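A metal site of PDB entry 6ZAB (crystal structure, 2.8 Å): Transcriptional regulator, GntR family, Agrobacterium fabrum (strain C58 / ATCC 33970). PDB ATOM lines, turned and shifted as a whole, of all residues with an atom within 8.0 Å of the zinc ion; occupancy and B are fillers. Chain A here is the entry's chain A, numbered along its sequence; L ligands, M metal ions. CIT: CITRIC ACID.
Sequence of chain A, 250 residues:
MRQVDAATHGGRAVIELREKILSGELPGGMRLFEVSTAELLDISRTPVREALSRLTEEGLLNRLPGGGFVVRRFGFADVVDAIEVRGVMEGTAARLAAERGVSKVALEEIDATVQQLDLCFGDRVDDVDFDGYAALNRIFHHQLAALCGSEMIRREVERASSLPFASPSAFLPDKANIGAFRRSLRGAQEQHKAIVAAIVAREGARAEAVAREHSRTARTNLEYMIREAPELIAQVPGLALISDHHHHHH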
ATOM      1  N   ARG A  86     -12.841  -9.551  18.934  1.00  0.00           N
ATOM      2  CA  ARG A  86     -11.728  -9.745  17.988  1.00  0.00           C
ATOM      3  C   ARG A  86     -12.013  -9.005  16.688  1.00  0.00           C
ATOM      4  O   ARG A  86     -11.161  -8.254  16.211  1.00  0.00           O
ATOM      5  CB  ARG A  86     -11.429 -11.225  17.721  1.00  0.00           C
ATOM      6  CG  ARG A  86     -10.419 -11.387  16.568  1.00  0.00           C
ATOM      7  CD  ARG A  86      -9.966 -12.807  16.373  1.00  0.00           C
ATOM      8  NE  ARG A  86     -11.069 -13.676  15.984  1.00  0.00           N
ATOM      9  CZ  ARG A  86     -11.236 -14.163  14.755  1.00  0.00           C
ATOM     10  NH1 ARG A  86     -10.359 -13.869  13.793  1.00  0.00           N
ATOM     11  NH2 ARG A  86     -12.252 -14.951  14.487  1.00  0.00           N
ATOM     12  N   GLU A  90      -9.608  -6.316  15.109  1.00  0.00           N
ATOM     13  CA  GLU A  90      -9.003  -6.572  13.806  1.00  0.00           C
ATOM     14  C   GLU A  90      -9.411  -5.488  12.795  1.00  0.00           C
ATOM     15  O   GLU A  90      -8.595  -5.066  11.957  1.00  0.00           O
ATOM     16  CB  GLU A  90      -9.388  -7.976  13.315  1.00  0.00           C
ATOM     17  CG  GLU A  90      -8.373  -9.019  13.767  1.00  0.00           C
ATOM     18  CD  GLU A  90      -8.691 -10.476  13.492  1.00  0.00           C
ATOM     19  OE1 GLU A  90      -9.761 -10.774  12.908  1.00  0.00           O
ATOM     20  OE2 GLU A  90      -7.849 -11.317  13.874  1.00  0.00           O
ATOM     21  N   LEU A 117      -1.244 -18.075   0.710  1.00  0.00           N
ATOM     22  CA  LEU A 117      -2.565 -18.571   1.088  1.00  0.00           C
ATOM     23  C   LEU A 117      -3.365 -18.969  -0.153  1.00  0.00           C
ATOM     24  O   LEU A 117      -4.174 -19.891  -0.061  1.00  0.00           O
ATOM     25  CB  LEU A 117      -3.334 -17.535   1.918  1.00  0.00           C
ATOM     26  CG  LEU A 117      -3.102 -17.525   3.426  1.00  0.00           C
ATOM     27  CD1 LEU A 117      -3.467 -16.194   4.016  1.00  0.00           C
ATOM     28  CD2 LEU A 117      -3.890 -18.617   4.118  1.00  0.00           C
ATOM     29  N   TYR A 133      -3.112 -23.842   5.364  1.00  0.00           N
ATOM     30  CA  TYR A 133      -3.912 -22.614   5.400  1.00  0.00           C
ATOM     31  C   TYR A 133      -3.911 -22.026   6.807  1.00  0.00           C
ATOM     32  O   TYR A 133      -3.387 -20.939   6.988  1.00  0.00           O
ATOM     33  CB  TYR A 133      -5.374 -22.889   4.928  1.00  0.00           C
ATOM     34  CG  TYR A 133      -6.305 -21.697   4.981  1.00  0.00           C
ATOM     35  CD1 TYR A 133      -7.035 -21.407   6.131  1.00  0.00           C
ATOM     36  CD2 TYR A 133      -6.531 -20.921   3.852  1.00  0.00           C
ATOM     37  CE1 TYR A 133      -7.913 -20.330   6.175  1.00  0.00           C
ATOM     38  CE2 TYR A 133      -7.405 -19.832   3.888  1.00  0.00           C
ATOM     39  CZ  TYR A 133      -8.100 -19.547   5.057  1.00  0.00           C
ATOM     40  OH  TYR A 133      -8.966 -18.480   5.093  1.00  0.00           O
ATOM     41  N   ALA A 134      -4.479 -22.771   7.791  1.00  0.00           N
ATOM     42  CA  ALA A 134      -4.591 -22.395   9.207  1.00  0.00           C
ATOM     43  C   ALA A 134      -3.298 -21.823   9.813  1.00  0.00           C
ATOM     44  O   ALA A 134      -3.365 -20.867  10.585  1.00  0.00           O
ATOM     45  CB  ALA A 134      -5.090 -23.587  10.021  1.00  0.00           C
ATOM     46  N   LEU A 136      -0.786 -20.358   7.999  1.00  0.00           N
ATOM     47  CA  LEU A 136      -0.549 -19.106   7.254  1.00  0.00           C
ATOM     48  C   LEU A 136      -1.551 -18.013   7.634  1.00  0.00           C
ATOM     49  O   LEU A 136      -1.206 -16.832   7.696  1.00  0.00           O
ATOM     50  CB  LEU A 136      -0.610 -19.347   5.739  1.00  0.00           C
ATOM     51  CG  LEU A 136       0.613 -19.996   5.084  1.00  0.00           C
ATOM     52  CD1 LEU A 136       0.221 -20.622   3.767  1.00  0.00           C
ATOM     53  CD2 LEU A 136       1.741 -18.977   4.877  1.00  0.00           C
ATOM     54  N   ASN A 137      -2.810 -18.426   7.869  1.00  0.00           N
ATOM     55  CA  ASN A 137      -3.935 -17.602   8.287  1.00  0.00           C
ATOM     56  C   ASN A 137      -3.555 -16.893   9.575  1.00  0.00           C
ATOM     57  O   ASN A 137      -3.692 -15.685   9.667  1.00  0.00           O
ATOM     58  CB  ASN A 137      -5.176 -18.464   8.462  1.00  0.00           C
ATOM     59  CG  ASN A 137      -6.274 -17.800   9.238  1.00  0.00           C
ATOM     60  OD1 ASN A 137      -6.920 -16.858   8.781  1.00  0.00           O
ATOM     61  ND2 ASN A 137      -6.502 -18.285  10.448  1.00  0.00           N
ATOM     62  N   ARG A 138      -2.993 -17.657  10.532  1.00  0.00           N
ATOM     63  CA  ARG A 138      -2.515 -17.107  11.794  1.00  0.00           C
ATOM     64  C   ARG A 138      -1.387 -16.088  11.564  1.00  0.00           C
ATOM     65  O   ARG A 138      -1.303 -15.120  12.318  1.00  0.00           O
ATOM     66  CB  ARG A 138      -2.077 -18.231  12.739  1.00  0.00           C
ATOM     67  CG  ARG A 138      -2.632 -18.125  14.168  1.00  0.00           C
ATOM     68  CD  ARG A 138      -2.041 -19.189  15.087  1.00  0.00           C
ATOM     69  NE  ARG A 138      -2.644 -20.523  14.881  1.00  0.00           N
ATOM     70  CZ  ARG A 138      -2.040 -21.549  14.277  1.00  0.00           C
ATOM     71  NH1 ARG A 138      -0.808 -21.418  13.809  1.00  0.00           N
ATOM     72  NH2 ARG A 138      -2.676 -22.709  14.146  1.00  0.00           N
ATOM     73  N   PHE A 140      -1.086 -14.086   8.796  1.00  0.00           N
ATOM     74  CA  PHE A 140      -1.804 -12.926   8.246  1.00  0.00           C
ATOM     75  C   PHE A 140      -2.323 -12.025   9.355  1.00  0.00           C
ATOM     76  O   PHE A 140      -1.991 -10.834   9.400  1.00  0.00           O
ATOM     77  CB  PHE A 140      -2.983 -13.408   7.369  1.00  0.00           C
ATOM     78  CG  PHE A 140      -3.832 -12.285   6.813  1.00  0.00           C
ATOM     79  CD1 PHE A 140      -3.435 -11.582   5.688  1.00  0.00           C
ATOM     80  CD2 PHE A 140      -5.036 -11.945   7.426  1.00  0.00           C
ATOM     81  CE1 PHE A 140      -4.227 -10.556   5.171  1.00  0.00           C
ATOM     82  CE2 PHE A 140      -5.805 -10.897   6.925  1.00  0.00           C
ATOM     83  CZ  PHE A 140      -5.411 -10.223   5.796  1.00  0.00           C
ATOM     84  N   HIS A 141      -3.103 -12.617  10.273  1.00  0.00           N
ATOM     85  CA  HIS A 141      -3.740 -11.944  11.390  1.00  0.00           C
ATOM     86  C   HIS A 141      -2.744 -11.246  12.311  1.00  0.00           C
ATOM     87  O   HIS A 141      -3.051 -10.171  12.838  1.00  0.00           O
ATOM     88  CB  HIS A 141      -4.641 -12.928  12.132  1.00  0.00           C
ATOM     89  CG  HIS A 141      -5.864 -13.231  11.330  1.00  0.00           C
ATOM     90  ND1 HIS A 141      -6.993 -12.449  11.421  1.00  0.00           N
ATOM     91  CD2 HIS A 141      -6.058 -14.158  10.365  1.00  0.00           C
ATOM     92  CE1 HIS A 141      -7.843 -12.951  10.544  1.00  0.00           C
ATOM     93  NE2 HIS A 141      -7.322 -13.981   9.888  1.00  0.00           N
ATOM     94  N   LEU A 144      -1.432  -8.169  10.196  1.00  0.00           N
ATOM     95  CA  LEU A 144      -2.503  -7.157  10.181  1.00  0.00           C
ATOM     96  C   LEU A 144      -2.543  -6.392  11.503  1.00  0.00           C
ATOM     97  O   LEU A 144      -2.724  -5.156  11.502  1.00  0.00           O
ATOM     98  CB  LEU A 144      -3.859  -7.848   9.901  1.00  0.00           C
ATOM     99  CG  LEU A 144      -5.162  -7.033  10.048  1.00  0.00           C
ATOM    100  CD1 LEU A 144      -5.206  -5.861   9.102  1.00  0.00           C
ATOM    101  CD2 LEU A 144      -6.367  -7.901   9.815  1.00  0.00           C
ATOM    102  N   PRO A 168      -7.643 -16.613  15.703  1.00  0.00           N
ATOM    103  CA  PRO A 168      -8.070 -16.584  14.288  1.00  0.00           C
ATOM    104  C   PRO A 168      -8.330 -17.987  13.718  1.00  0.00           C
ATOM    105  O   PRO A 168      -9.456 -18.261  13.303  1.00  0.00           O
ATOM    106  CB  PRO A 168      -6.942 -15.844  13.570  1.00  0.00           C
ATOM    107  CG  PRO A 168      -6.157 -15.181  14.637  1.00  0.00           C
ATOM    108  CD  PRO A 168      -6.287 -16.031  15.848  1.00  0.00           C
ATOM    109  N   SER A 169      -7.322 -18.876  13.775  1.00  0.00           N
ATOM    110  CA  SER A 169      -7.442 -20.263  13.285  1.00  0.00           C
ATOM    111  C   SER A 169      -7.883 -21.218  14.406  1.00  0.00           C
ATOM    112  O   SER A 169      -7.248 -22.254  14.647  1.00  0.00           O
ATOM    113  CB  SER A 169      -6.147 -20.710  12.602  1.00  0.00           C
ATOM    114  OG  SER A 169      -5.007 -20.483  13.413  1.00  0.00           O
ATOM    115  N   LEU A 172     -10.547 -24.066  12.795  1.00  0.00           N
ATOM    116  CA  LEU A 172      -9.805 -24.784  11.758  1.00  0.00           C
ATOM    117  C   LEU A 172      -9.030 -26.023  12.310  1.00  0.00           C
ATOM    118  O   LEU A 172      -7.877 -26.231  11.915  1.00  0.00           O
ATOM    119  CB  LEU A 172      -8.869 -23.830  10.990  1.00  0.00           C
ATOM    120  CG  LEU A 172      -9.515 -22.797  10.080  1.00  0.00           C
ATOM    121  CD1 LEU A 172      -8.497 -21.827   9.540  1.00  0.00           C
ATOM    122  CD2 LEU A 172     -10.278 -23.455   8.944  1.00  0.00           C
ATOM    123  N   LEU A 185     -13.686 -21.362   3.366  1.00  0.00           N
ATOM    124  CA  LEU A 185     -12.312 -20.853   3.273  1.00  0.00           C
ATOM    125  C   LEU A 185     -11.964 -20.152   1.977  1.00  0.00           C
ATOM    126  O   LEU A 185     -11.105 -19.264   1.982  1.00  0.00           O
ATOM    127  CB  LEU A 185     -11.282 -21.955   3.541  1.00  0.00           C
ATOM    128  CG  LEU A 185     -11.232 -22.529   4.955  1.00  0.00           C
ATOM    129  CD1 LEU A 185      -9.966 -23.313   5.139  1.00  0.00           C
ATOM    130  CD2 LEU A 185     -11.338 -21.452   6.010  1.00  0.00           C
ATOM    131  N   ALA A 188     -13.146 -16.750   2.618  1.00  0.00           N
ATOM    132  CA  ALA A 188     -12.349 -16.097   3.652  1.00  0.00           C
ATOM    133  C   ALA A 188     -11.044 -15.572   3.074  1.00  0.00           C
ATOM    134  O   ALA A 188     -10.523 -14.575   3.561  1.00  0.00           O
ATOM    135  CB  ALA A 188     -12.072 -17.060   4.783  1.00  0.00           C
ATOM    136  N   GLN A 189     -10.544 -16.212   2.015  1.00  0.00           N
ATOM    137  CA  GLN A 189      -9.339 -15.763   1.341  1.00  0.00           C
ATOM    138  C   GLN A 189      -9.629 -14.463   0.598  1.00  0.00           C
ATOM    139  O   GLN A 189      -8.768 -13.588   0.550  1.00  0.00           O
ATOM    140  CB  GLN A 189      -8.757 -16.843   0.410  1.00  0.00           C
ATOM    141  CG  GLN A 189      -7.430 -16.476  -0.275  1.00  0.00           C
ATOM    142  CD  GLN A 189      -6.348 -15.951   0.657  1.00  0.00           C
ATOM    143  OE1 GLN A 189      -6.246 -16.330   1.830  1.00  0.00           O
ATOM    144  NE2 GLN A 189      -5.500 -15.072   0.131  1.00  0.00           N
ATOM    145  N   GLN A 191     -11.828 -12.225   1.603  1.00  0.00           N
ATOM    146  CA  GLN A 191     -11.910 -11.258   2.690  1.00  0.00           C
ATOM    147  C   GLN A 191     -10.506 -10.789   3.058  1.00  0.00           C
ATOM    148  O   GLN A 191     -10.306  -9.579   3.232  1.00  0.00           O
ATOM    149  CB  GLN A 191     -12.619 -11.873   3.901  1.00  0.00           C
ATOM    150  CG  GLN A 191     -14.082 -12.184   3.661  1.00  0.00           C
ATOM    151  CD  GLN A 191     -14.802 -12.558   4.922  1.00  0.00           C
ATOM    152  OE1 GLN A 191     -14.504 -13.576   5.571  1.00  0.00           O
ATOM    153  NE2 GLN A 191     -15.797 -11.765   5.293  1.00  0.00           N
ATOM    154  N   HIS A 192      -9.526 -11.717   3.099  1.00  0.00           N
ATOM    155  CA  HIS A 192      -8.114 -11.427   3.364  1.00  0.00           C
ATOM    156  C   HIS A 192      -7.564 -10.482   2.287  1.00  0.00           C
ATOM    157  O   HIS A 192      -6.870  -9.517   2.621  1.00  0.00           O
ATOM    158  CB  HIS A 192      -7.290 -12.723   3.393  1.00  0.00           C
ATOM    159  CG  HIS A 192      -7.460 -13.578   4.616  1.00  0.00           C
ATOM    160  ND1 HIS A 192      -7.063 -14.907   4.618  1.00  0.00           N
ATOM    161  CD2 HIS A 192      -7.921 -13.266   5.848  1.00  0.00           C
ATOM    162  CE1 HIS A 192      -7.315 -15.348   5.840  1.00  0.00           C
ATOM    163  NE2 HIS A 192      -7.815 -14.398   6.618  1.00  0.00           N
ATOM    164  N   ILE A 195      -9.259  -6.951   2.665  1.00  0.00           N
ATOM    165  CA  ILE A 195      -8.689  -6.224   3.800  1.00  0.00           C
ATOM    166  C   ILE A 195      -7.475  -5.433   3.323  1.00  0.00           C
ATOM    167  O   ILE A 195      -7.451  -4.209   3.442  1.00  0.00           O
ATOM    168  CB  ILE A 195      -8.385  -7.154   5.013  1.00  0.00           C
ATOM    169  CG1 ILE A 195      -9.689  -7.564   5.735  1.00  0.00           C
ATOM    170  CG2 ILE A 195      -7.429  -6.491   6.017  1.00  0.00           C
ATOM    171  CD1 ILE A 195      -9.596  -8.813   6.623  1.00  0.00           C
ATOM    172  N   HIS A 214     -15.138 -10.673   8.625  1.00  0.00           N
ATOM    173  CA  HIS A 214     -14.261 -11.823   8.544  1.00  0.00           C
ATOM    174  C   HIS A 214     -14.380 -12.640   9.828  1.00  0.00           C
ATOM    175  O   HIS A 214     -14.617 -13.831   9.736  1.00  0.00           O
ATOM    176  CB  HIS A 214     -12.823 -11.383   8.286  1.00  0.00           C
ATOM    177  CG  HIS A 214     -11.909 -12.520   7.980  1.00  0.00           C
ATOM    178  ND1 HIS A 214     -12.024 -13.242   6.811  1.00  0.00           N
ATOM    179  CD2 HIS A 214     -10.870 -13.019   8.700  1.00  0.00           C
ATOM    180  CE1 HIS A 214     -11.071 -14.161   6.852  1.00  0.00           C
ATOM    181  NE2 HIS A 214     -10.347 -14.061   7.966  1.00  0.00           N
ATOM    182  N   SER A 215     -14.312 -11.994  11.010  1.00  0.00           N
ATOM    183  CA  SER A 215     -14.442 -12.686  12.299  1.00  0.00           C
ATOM    184  C   SER A 215     -15.827 -13.344  12.420  1.00  0.00           C
ATOM    185  O   SER A 215     -15.928 -14.421  13.005  1.00  0.00           O
ATOM    186  CB  SER A 215     -14.175 -11.747  13.471  1.00  0.00           C
ATOM    187  OG  SER A 215     -15.355 -11.094  13.905  1.00  0.00           O
ATOM    188  N   THR A 217     -17.270 -15.057  10.308  1.00  0.00           N
ATOM    189  CA  THR A 217     -17.088 -16.377   9.668  1.00  0.00           C
ATOM    190  C   THR A 217     -17.004 -17.454  10.773  1.00  0.00           C
ATOM    191  O   THR A 217     -17.681 -18.467  10.675  1.00  0.00           O
ATOM    192  CB  THR A 217     -15.849 -16.364   8.713  1.00  0.00           C
ATOM    193  OG1 THR A 217     -16.166 -15.637   7.528  1.00  0.00           O
ATOM    194  CG2 THR A 217     -15.345 -17.758   8.329  1.00  0.00           C
HETATM  195  C1  CIT L   1     -12.135 -15.687  11.118  1.00  0.00           C
HETATM  196  O1  CIT L   1     -11.123 -14.884  11.292  1.00  0.00           O
HETATM  197  O2  CIT L   1     -13.066 -15.775  11.893  1.00  0.00           O
HETATM  198  C2  CIT L   1     -12.063 -16.492   9.852  1.00  0.00           C
HETATM  199  C3  CIT L   1     -10.906 -17.508   9.727  1.00  0.00           C
HETATM  200  O7  CIT L   1      -9.685 -16.846  10.070  1.00  0.00           O
HETATM  201  C4  CIT L   1     -11.045 -18.695  10.700  1.00  0.00           C
HETATM  202  C5  CIT L   1     -12.322 -19.478  10.721  1.00  0.00           C
HETATM  203  O3  CIT L   1     -12.376 -20.413   9.816  1.00  0.00           O
HETATM  204  O4  CIT L   1     -13.219 -19.274  11.513  1.00  0.00           O
HETATM  205  C6  CIT L   1     -10.805 -17.984   8.283  1.00  0.00           C
HETATM  206  O5  CIT L   1      -9.815 -17.811   7.597  1.00  0.00           O
HETATM  207  O6  CIT L   1     -11.889 -18.587   7.857  1.00  0.00           O
HETATM  208 ZN    ZN M   1      -8.505 -15.468   8.509  1.00  0.00          ZN
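ND2 of Asn 137 lies close to N of Ser 169, 3.5 Å away. ND1 of His 192 sits at hydrogen-bond distance from OE1 of Gln 189, at 3.2 Å. ND1 of His 141 sits at hydrogen-bond distance from OE2 of Glu 90 (2.8 Å). A ring nitrogen (ND1) of His 214 lies within hydrogen-bond range of the side-chain amide oxygen (OE1) of Gln 191, at 2.8 Å. The side-chain hydroxyl (OG1) of Thr 217 lies close to the backbone carbonyl oxygen (O) of His 214 (3.2 Å).
The zinc ion is bound by the side-chain amide oxygen of Asn 137 (2.1 Å), a ring nitrogen (NE2) of His 192 (2.3 Å), a ring nitrogen (NE2) of His 141 (2.3 Å), a ring nitrogen (NE2) of His 214 (2.4 Å) and an oxygen (O7) of the ligand (2.4 Å). Slightly farther from the zinc ion lies an oxygen (O5) of the ligand (2.8 Å).
Within 4 Å of the zinc ion: Asn 137, His 141, His 192 and His 214. The nearest printed residue that does not touch the zinc ion is Tyr 133 (4.6 Å).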
